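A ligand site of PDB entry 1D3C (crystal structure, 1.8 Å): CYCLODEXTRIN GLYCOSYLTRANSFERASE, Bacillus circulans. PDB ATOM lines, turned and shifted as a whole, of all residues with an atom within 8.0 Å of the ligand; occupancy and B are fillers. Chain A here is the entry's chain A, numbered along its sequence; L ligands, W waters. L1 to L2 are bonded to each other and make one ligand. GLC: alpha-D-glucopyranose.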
ATOM      1  N   TYR A 301      36.544  18.408 -16.600  1.00  0.00           N
ATOM      2  CA  TYR A 301      37.091  19.686 -16.168  1.00  0.00           C
ATOM      3  C   TYR A 301      38.161  20.133 -17.154  1.00  0.00           C
ATOM      4  O   TYR A 301      38.372  21.323 -17.361  1.00  0.00           O
ATOM      5  CB  TYR A 301      37.645  19.606 -14.755  1.00  0.00           C
ATOM      6  CG  TYR A 301      36.579  19.343 -13.728  1.00  0.00           C
ATOM      7  CD1 TYR A 301      35.699  20.348 -13.346  1.00  0.00           C
ATOM      8  CD2 TYR A 301      36.387  18.079 -13.215  1.00  0.00           C
ATOM      9  CE1 TYR A 301      34.687  20.102 -12.430  1.00  0.00           C
ATOM     10  CE2 TYR A 301      35.382  17.818 -12.301  1.00  0.00           C
ATOM     11  CZ  TYR A 301      34.536  18.832 -11.914  1.00  0.00           C
ATOM     12  OH  TYR A 301      33.531  18.579 -11.007  1.00  0.00           O
ATOM     13  N   LYS A 304      36.185  21.370 -20.231  1.00  0.00           N
ATOM     14  CA  LYS A 304      35.659  22.691 -19.894  1.00  0.00           C
ATOM     15  C   LYS A 304      36.768  23.724 -19.941  1.00  0.00           C
ATOM     16  O   LYS A 304      36.594  24.810 -20.479  1.00  0.00           O
ATOM     17  CB  LYS A 304      35.004  22.678 -18.513  1.00  0.00           C
ATOM     18  CG  LYS A 304      34.773  24.053 -17.947  1.00  0.00           C
ATOM     19  CD  LYS A 304      34.285  23.979 -16.507  1.00  0.00           C
ATOM     20  CE  LYS A 304      34.647  25.232 -15.729  1.00  0.00           C
ATOM     21  NZ  LYS A 304      33.442  25.988 -15.306  1.00  0.00           N
ATOM     22  N   GLN A 410      28.875  28.015 -22.882  1.00  0.00           N
ATOM     23  CA  GLN A 410      28.889  28.129 -21.426  1.00  0.00           C
ATOM     24  C   GLN A 410      28.630  26.821 -20.727  1.00  0.00           C
ATOM     25  O   GLN A 410      27.703  26.086 -21.082  1.00  0.00           O
ATOM     26  CB  GLN A 410      27.896  29.169 -20.943  1.00  0.00           C
ATOM     27  CG  GLN A 410      27.908  29.354 -19.454  1.00  0.00           C
ATOM     28  CD  GLN A 410      26.860  30.330 -18.988  1.00  0.00           C
ATOM     29  OE1 GLN A 410      25.930  30.668 -19.725  1.00  0.00           O
ATOM     30  NE2 GLN A 410      27.013  30.794 -17.750  1.00  0.00           N
ATOM     31  N   GLU A 411      29.437  26.536 -19.716  1.00  0.00           N
ATOM     32  CA  GLU A 411      29.271  25.334 -18.926  1.00  0.00           C
ATOM     33  C   GLU A 411      28.051  25.524 -18.019  1.00  0.00           C
ATOM     34  O   GLU A 411      27.962  26.526 -17.304  1.00  0.00           O
ATOM     35  CB  GLU A 411      30.529  25.070 -18.110  1.00  0.00           C
ATOM     36  CG  GLU A 411      30.367  23.969 -17.101  1.00  0.00           C
ATOM     37  CD  GLU A 411      29.949  24.481 -15.755  1.00  0.00           C
ATOM     38  OE1 GLU A 411      30.742  25.207 -15.133  1.00  0.00           O
ATOM     39  OE2 GLU A 411      28.780  24.219 -15.362  1.00  0.00           O
ATOM     40  N   ARG A 412      27.106  24.591 -18.064  1.00  0.00           N
ATOM     41  CA  ARG A 412      25.873  24.685 -17.262  1.00  0.00           C
ATOM     42  C   ARG A 412      25.811  23.632 -16.153  1.00  0.00           C
ATOM     43  O   ARG A 412      25.167  23.840 -15.115  1.00  0.00           O
ATOM     44  CB  ARG A 412      24.642  24.590 -18.153  1.00  0.00           C
ATOM     45  CG  ARG A 412      24.462  25.765 -19.103  1.00  0.00           C
ATOM     46  CD  ARG A 412      24.288  27.071 -18.352  1.00  0.00           C
ATOM     47  NE  ARG A 412      23.455  28.017 -19.100  1.00  0.00           N
ATOM     48  CZ  ARG A 412      22.858  29.065 -18.561  1.00  0.00           C
ATOM     49  NH1 ARG A 412      22.991  29.331 -17.270  1.00  0.00           N
ATOM     50  NH2 ARG A 412      22.121  29.870 -19.316  1.00  0.00           N
ATOM     51  N   TRP A 413      26.434  22.488 -16.382  1.00  0.00           N
ATOM     52  CA  TRP A 413      26.452  21.392 -15.410  1.00  0.00           C
ATOM     53  C   TRP A 413      27.699  20.576 -15.664  1.00  0.00           C
ATOM     54  O   TRP A 413      28.075  20.351 -16.818  1.00  0.00           O
ATOM     55  CB  TRP A 413      25.211  20.517 -15.558  1.00  0.00           C
ATOM     56  CG  TRP A 413      24.751  19.872 -14.265  1.00  0.00           C
ATOM     57  CD1 TRP A 413      23.789  20.335 -13.422  1.00  0.00           C
ATOM     58  CD2 TRP A 413      25.229  18.643 -13.706  1.00  0.00           C
ATOM     59  NE1 TRP A 413      23.648  19.472 -12.345  1.00  0.00           N
ATOM     60  CE2 TRP A 413      24.517  18.428 -12.498  1.00  0.00           C
ATOM     61  CE3 TRP A 413      26.191  17.713 -14.092  1.00  0.00           C
ATOM     62  CZ2 TRP A 413      24.747  17.320 -11.690  1.00  0.00           C
ATOM     63  CZ3 TRP A 413      26.411  16.607 -13.282  1.00  0.00           C
ATOM     64  CH2 TRP A 413      25.683  16.416 -12.104  1.00  0.00           C
ATOM     65  N   ILE A 414      28.368  20.159 -14.600  1.00  0.00           N
ATOM     66  CA  ILE A 414      29.609  19.428 -14.773  1.00  0.00           C
ATOM     67  C   ILE A 414      30.083  18.642 -13.566  1.00  0.00           C
ATOM     68  O   ILE A 414      29.871  19.016 -12.421  1.00  0.00           O
ATOM     69  CB  ILE A 414      30.745  20.388 -15.194  1.00  0.00           C
ATOM     70  CG1 ILE A 414      31.995  19.589 -15.552  1.00  0.00           C
ATOM     71  CG2 ILE A 414      31.034  21.386 -14.087  1.00  0.00           C
ATOM     72  CD1 ILE A 414      33.230  20.458 -15.741  1.00  0.00           C
ATOM     73  N   ASN A 415      30.732  17.524 -13.860  1.00  0.00           N
ATOM     74  CA  ASN A 415      31.410  16.694 -12.868  1.00  0.00           C
ATOM     75  C   ASN A 415      32.475  15.901 -13.644  1.00  0.00           C
ATOM     76  O   ASN A 415      32.771  16.251 -14.790  1.00  0.00           O
ATOM     77  CB  ASN A 415      30.450  15.842 -12.005  1.00  0.00           C
ATOM     78  CG  ASN A 415      29.770  14.704 -12.773  1.00  0.00           C
ATOM     79  OD1 ASN A 415      30.208  14.319 -13.859  1.00  0.00           O
ATOM     80  ND2 ASN A 415      28.736  14.112 -12.167  1.00  0.00           N
ATOM     81  N   ASN A 416      33.106  14.907 -13.025  1.00  0.00           N
ATOM     82  CA  ASN A 416      34.174  14.162 -13.703  1.00  0.00           C
ATOM     83  C   ASN A 416      33.806  13.681 -15.094  1.00  0.00           C
ATOM     84  O   ASN A 416      34.568  13.834 -16.033  1.00  0.00           O
ATOM     85  CB  ASN A 416      34.608  12.954 -12.872  1.00  0.00           C
ATOM     86  CG  ASN A 416      35.648  13.301 -11.851  1.00  0.00           C
ATOM     87  OD1 ASN A 416      36.041  14.451 -11.707  1.00  0.00           O
ATOM     88  ND2 ASN A 416      36.061  12.306 -11.082  1.00  0.00           N
ATOM     89  N   VAL A 418      30.505  14.192 -16.569  1.00  0.00           N
ATOM     90  CA  VAL A 418      29.385  14.861 -17.208  1.00  0.00           C
ATOM     91  C   VAL A 418      29.670  16.294 -17.590  1.00  0.00           C
ATOM     92  O   VAL A 418      30.192  17.075 -16.806  1.00  0.00           O
ATOM     93  CB  VAL A 418      28.125  14.849 -16.309  1.00  0.00           C
ATOM     94  CG1 VAL A 418      27.000  15.627 -16.976  1.00  0.00           C
ATOM     95  CG2 VAL A 418      27.692  13.431 -16.008  1.00  0.00           C
ATOM     96  N   LEU A 419      29.274  16.663 -18.809  1.00  0.00           N
ATOM     97  CA  LEU A 419      29.381  18.036 -19.233  1.00  0.00           C
ATOM     98  C   LEU A 419      28.132  18.468 -19.952  1.00  0.00           C
ATOM     99  O   LEU A 419      27.738  17.874 -20.953  1.00  0.00           O
ATOM    100  CB  LEU A 419      30.593  18.304 -20.124  1.00  0.00           C
ATOM    101  CG  LEU A 419      30.701  19.791 -20.525  1.00  0.00           C
ATOM    102  CD1 LEU A 419      31.014  20.676 -19.321  1.00  0.00           C
ATOM    103  CD2 LEU A 419      31.713  19.998 -21.636  1.00  0.00           C
ATOM    104  N   ILE A 420      27.508  19.498 -19.428  1.00  0.00           N
ATOM    105  CA  ILE A 420      26.326  20.047 -20.042  1.00  0.00           C
ATOM    106  C   ILE A 420      26.638  21.489 -20.373  1.00  0.00           C
ATOM    107  O   ILE A 420      26.879  22.314 -19.498  1.00  0.00           O
ATOM    108  CB  ILE A 420      25.108  19.929 -19.133  1.00  0.00           C
ATOM    109  CG1 ILE A 420      24.809  18.457 -18.852  1.00  0.00           C
ATOM    110  CG2 ILE A 420      23.904  20.610 -19.776  1.00  0.00           C
ATOM    111  CD1 ILE A 420      23.630  18.248 -17.915  1.00  0.00           C
ATOM    112  N   SER A 443      22.715  11.749 -12.114  1.00  0.00           N
ATOM    113  CA  SER A 443      21.500  12.450 -11.736  1.00  0.00           C
ATOM    114  C   SER A 443      21.698  13.940 -11.905  1.00  0.00           C
ATOM    115  O   SER A 443      22.502  14.555 -11.198  1.00  0.00           O
ATOM    116  CB  SER A 443      21.113  12.127 -10.304  1.00  0.00           C
ATOM    117  OG  SER A 443      20.962  10.730 -10.127  1.00  0.00           O
ATOM    118  N   ILE A 444      20.971  14.526 -12.846  1.00  0.00           N
ATOM    119  CA  ILE A 444      21.104  15.935 -13.127  1.00  0.00           C
ATOM    120  C   ILE A 444      20.036  16.781 -12.458  1.00  0.00           C
ATOM    121  O   ILE A 444      18.885  16.807 -12.878  1.00  0.00           O
ATOM    122  CB  ILE A 444      21.084  16.216 -14.637  1.00  0.00           C
ATOM    123  CG1 ILE A 444      22.083  15.296 -15.365  1.00  0.00           C
ATOM    124  CG2 ILE A 444      21.403  17.678 -14.916  1.00  0.00           C
ATOM    125  CD1 ILE A 444      23.469  15.319 -14.773  1.00  0.00           C
ATOM    126  N   SER A 445      20.447  17.493 -11.418  1.00  0.00           N
ATOM    127  CA  SER A 445      19.572  18.389 -10.720  1.00  0.00           C
ATOM    128  C   SER A 445      20.282  19.731 -10.618  1.00  0.00           C
ATOM    129  O   SER A 445      21.511  19.783 -10.607  1.00  0.00           O
ATOM    130  CB  SER A 445      19.203  17.844  -9.344  1.00  0.00           C
ATOM    131  OG  SER A 445      20.328  17.791  -8.499  1.00  0.00           O
ATOM    132  N   GLY A 446      19.514  20.801 -10.633  1.00  0.00           N
ATOM    133  CA  GLY A 446      20.084  22.142 -10.543  1.00  0.00           C
ATOM    134  C   GLY A 446      20.538  22.718 -11.897  1.00  0.00           C
ATOM    135  O   GLY A 446      21.209  23.747 -11.929  1.00  0.00           O
ATOM    136  N   LEU A 447      20.179  22.065 -12.999  1.00  0.00           N
ATOM    137  CA  LEU A 447      20.573  22.576 -14.311  1.00  0.00           C
ATOM    138  C   LEU A 447      19.756  23.791 -14.700  1.00  0.00           C
ATOM    139  O   LEU A 447      18.524  23.732 -14.719  1.00  0.00           O
ATOM    140  CB  LEU A 447      20.439  21.521 -15.400  1.00  0.00           C
ATOM    141  CG  LEU A 447      20.622  22.100 -16.817  1.00  0.00           C
ATOM    142  CD1 LEU A 447      22.079  22.483 -17.071  1.00  0.00           C
ATOM    143  CD2 LEU A 447      20.110  21.131 -17.873  1.00  0.00           C
ATOM    144  N   VAL A 448      20.433  24.883 -15.025  1.00  0.00           N
ATOM    145  CA  VAL A 448      19.773  26.098 -15.452  1.00  0.00           C
ATOM    146  C   VAL A 448      20.203  26.429 -16.881  1.00  0.00           C
ATOM    147  O   VAL A 448      21.382  26.331 -17.225  1.00  0.00           O
ATOM    148  CB  VAL A 448      20.095  27.274 -14.527  1.00  0.00           C
ATOM    149  CG1 VAL A 448      19.672  28.583 -15.186  1.00  0.00           C
ATOM    150  CG2 VAL A 448      19.408  27.102 -13.183  1.00  0.00           C
ATOM    151  N   THR A 449      19.226  26.783 -17.713  1.00  0.00           N
ATOM    152  CA  THR A 449      19.490  27.072 -19.120  1.00  0.00           C
ATOM    153  C   THR A 449      18.840  28.365 -19.581  1.00  0.00           C
ATOM    154  O   THR A 449      18.078  28.988 -18.844  1.00  0.00           O
ATOM    155  CB  THR A 449      18.966  25.936 -19.999  1.00  0.00           C
ATOM    156  OG1 THR A 449      17.560  26.121 -20.217  1.00  0.00           O
ATOM    157  CG2 THR A 449      19.177  24.585 -19.326  1.00  0.00           C
ATOM    158  N   ALA A 476      15.099  26.939 -15.355  1.00  0.00           N
ATOM    159  CA  ALA A 476      15.523  25.812 -14.523  1.00  0.00           C
ATOM    160  C   ALA A 476      14.912  24.501 -15.012  1.00  0.00           C
ATOM    161  O   ALA A 476      13.691  24.401 -15.154  1.00  0.00           O
ATOM    162  CB  ALA A 476      15.144  26.052 -13.065  1.00  0.00           C
HETATM  163  C1  GLC L   1      26.229  19.770  -9.146  1.00  0.00           C
HETATM  164  C2  GLC L   1      27.044  19.908 -10.396  1.00  0.00           C
HETATM  165  C3  GLC L   1      27.263  21.364 -10.728  1.00  0.00           C
HETATM  166  C4  GLC L   1      25.913  22.065 -10.769  1.00  0.00           C
HETATM  167  C5  GLC L   1      25.134  21.863  -9.474  1.00  0.00           C
HETATM  168  C6  GLC L   1      23.731  22.417  -9.597  1.00  0.00           C
HETATM  169  O1  GLC L   1      26.957  20.259  -8.072  1.00  0.00           O
HETATM  170  O2  GLC L   1      28.311  19.266 -10.233  1.00  0.00           O
HETATM  171  O3  GLC L   1      27.926  21.466 -11.981  1.00  0.00           O
HETATM  172  O4  GLC L   1      26.153  23.464 -10.970  1.00  0.00           O
HETATM  173  O5  GLC L   1      24.986  20.452  -9.314  1.00  0.00           O
HETATM  174  O6  GLC L   1      23.167  22.550  -8.292  1.00  0.00           O
HETATM  175  C1  GLC L   2      25.768  24.025 -12.203  1.00  0.00           C
HETATM  176  C2  GLC L   2      26.913  24.885 -12.691  1.00  0.00           C
HETATM  177  C3  GLC L   2      27.123  26.048 -11.750  1.00  0.00           C
HETATM  178  C4  GLC L   2      25.833  26.798 -11.502  1.00  0.00           C
HETATM  179  C5  GLC L   2      24.718  25.850 -11.087  1.00  0.00           C
HETATM  180  C6  GLC L   2      23.391  26.553 -11.052  1.00  0.00           C
HETATM  181  O2  GLC L   2      28.090  24.096 -12.769  1.00  0.00           O
HETATM  182  O3  GLC L   2      28.058  26.981 -12.306  1.00  0.00           O
HETATM  183  O4  GLC L   2      25.978  27.695 -10.411  1.00  0.00           O
HETATM  184  O5  GLC L   2      24.590  24.790 -12.045  1.00  0.00           O
HETATM  185  O6  GLC L   2      22.352  25.741 -10.510  1.00  0.00           O
HETATM  186  O   HOH W   1      23.137  25.473 -14.386  1.00  0.00           O
HETATM  187  O   HOH W   2      28.550  17.187  -8.538  1.00  0.00           O
HETATM  188  O   HOH W   3      28.224  29.174 -10.579  1.00  0.00           O
HETATM  189  O   HOH W   4      31.356  20.057 -10.415  1.00  0.00           O
HETATM  190  O   HOH W   5      19.712  26.181 -10.108  1.00  0.00           O
HETATM  191  O   HOH W   6      22.619  19.916  -8.160  1.00  0.00           O
HETATM  192  O   HOH W   7      27.042  27.418 -14.942  1.00  0.00           O
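The backbone carbonyl oxygen (O) of Arg 412 lies close to an oxygen (O5) of GLC L2 (3.3 Å). Merely in contact with the ligand: Ser 445 (3.6 Å). Hydrophobic or aromatic side chains that line the ligand: Trp 413 and Ile 414. Of the 20 residues printed, 6 come within 4 Å of the ligand. The nearest printed residue that does not touch the ligand is Val 448 (4.2 Å).
An oxygen (O2) of GLC L1 lies within hydrogen-bond range of the backbone carbonyl oxygen (O) of Ile 414, 2.7 Å away. An oxygen (O2) of GLC L2 is in hydrogen-bond range of the side-chain carboxylate (OE2) of Glu 411 (2.7 Å). The backbone carbonyl oxygen (O) of Gly 446 sits at hydrogen-bond distance from an oxygen (O6) of GLC L2, at 2.7 Å. The indole nitrogen of Trp 413 sits at hydrogen-bond distance from an oxygen (O5) of GLC L1 (3.5 Å). The backbone NH (N) of Ile 414 sits at hydrogen-bond distance from an oxygen (O3) of GLC L1, 3.0 Å away.
Water W6 lies within hydrogen-bond range of O5 of GLC L1 (2.7 Å) and O of Ser 445 (2.7 Å). Water W5 bridges an oxygen (O6) of GLC L2 and the backbone carbonyl oxygen (O) of Gly 446. Water W1 lies within hydrogen-bond range of O of Arg 412 (2.7 Å), O5 of GLC L2 (2.8 Å) and N of Val 448 (2.8 Å). Water W7 bridges O of Glu 411 (2.7 Å) and O3 of GLC L2 (2.9 Å). Water W4 lies within hydrogen-bond range of OH of Tyr 301 (2.7 Å), O of Ile 414 (2.7 Å) and O2 of GLC L1 (3.2 Å).
The backbone NH (N) of Arg 412 is in hydrogen-bond range of the backbone carbonyl oxygen (O) of Ile 420 (2.7 Å). OE2 of Glu 411 sits at hydrogen-bond distance from N of Trp 413, 3.1 Å away. The backbone carbonyl oxygen (O) of Ser 445 is in hydrogen-bond range of the indole nitrogen (NE1) of Trp 413, at 2.8 Å. O of Trp 413 is in hydrogen-bond range of N of Ile 420, at 2.8 Å. O of Val 448 lies close to NE of Arg 412 (3.3 Å). The side-chain carboxylate (OE1) of Glu 411 lies within salt-bridge range of the side-chain amino group (NZ) of Lys 304.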
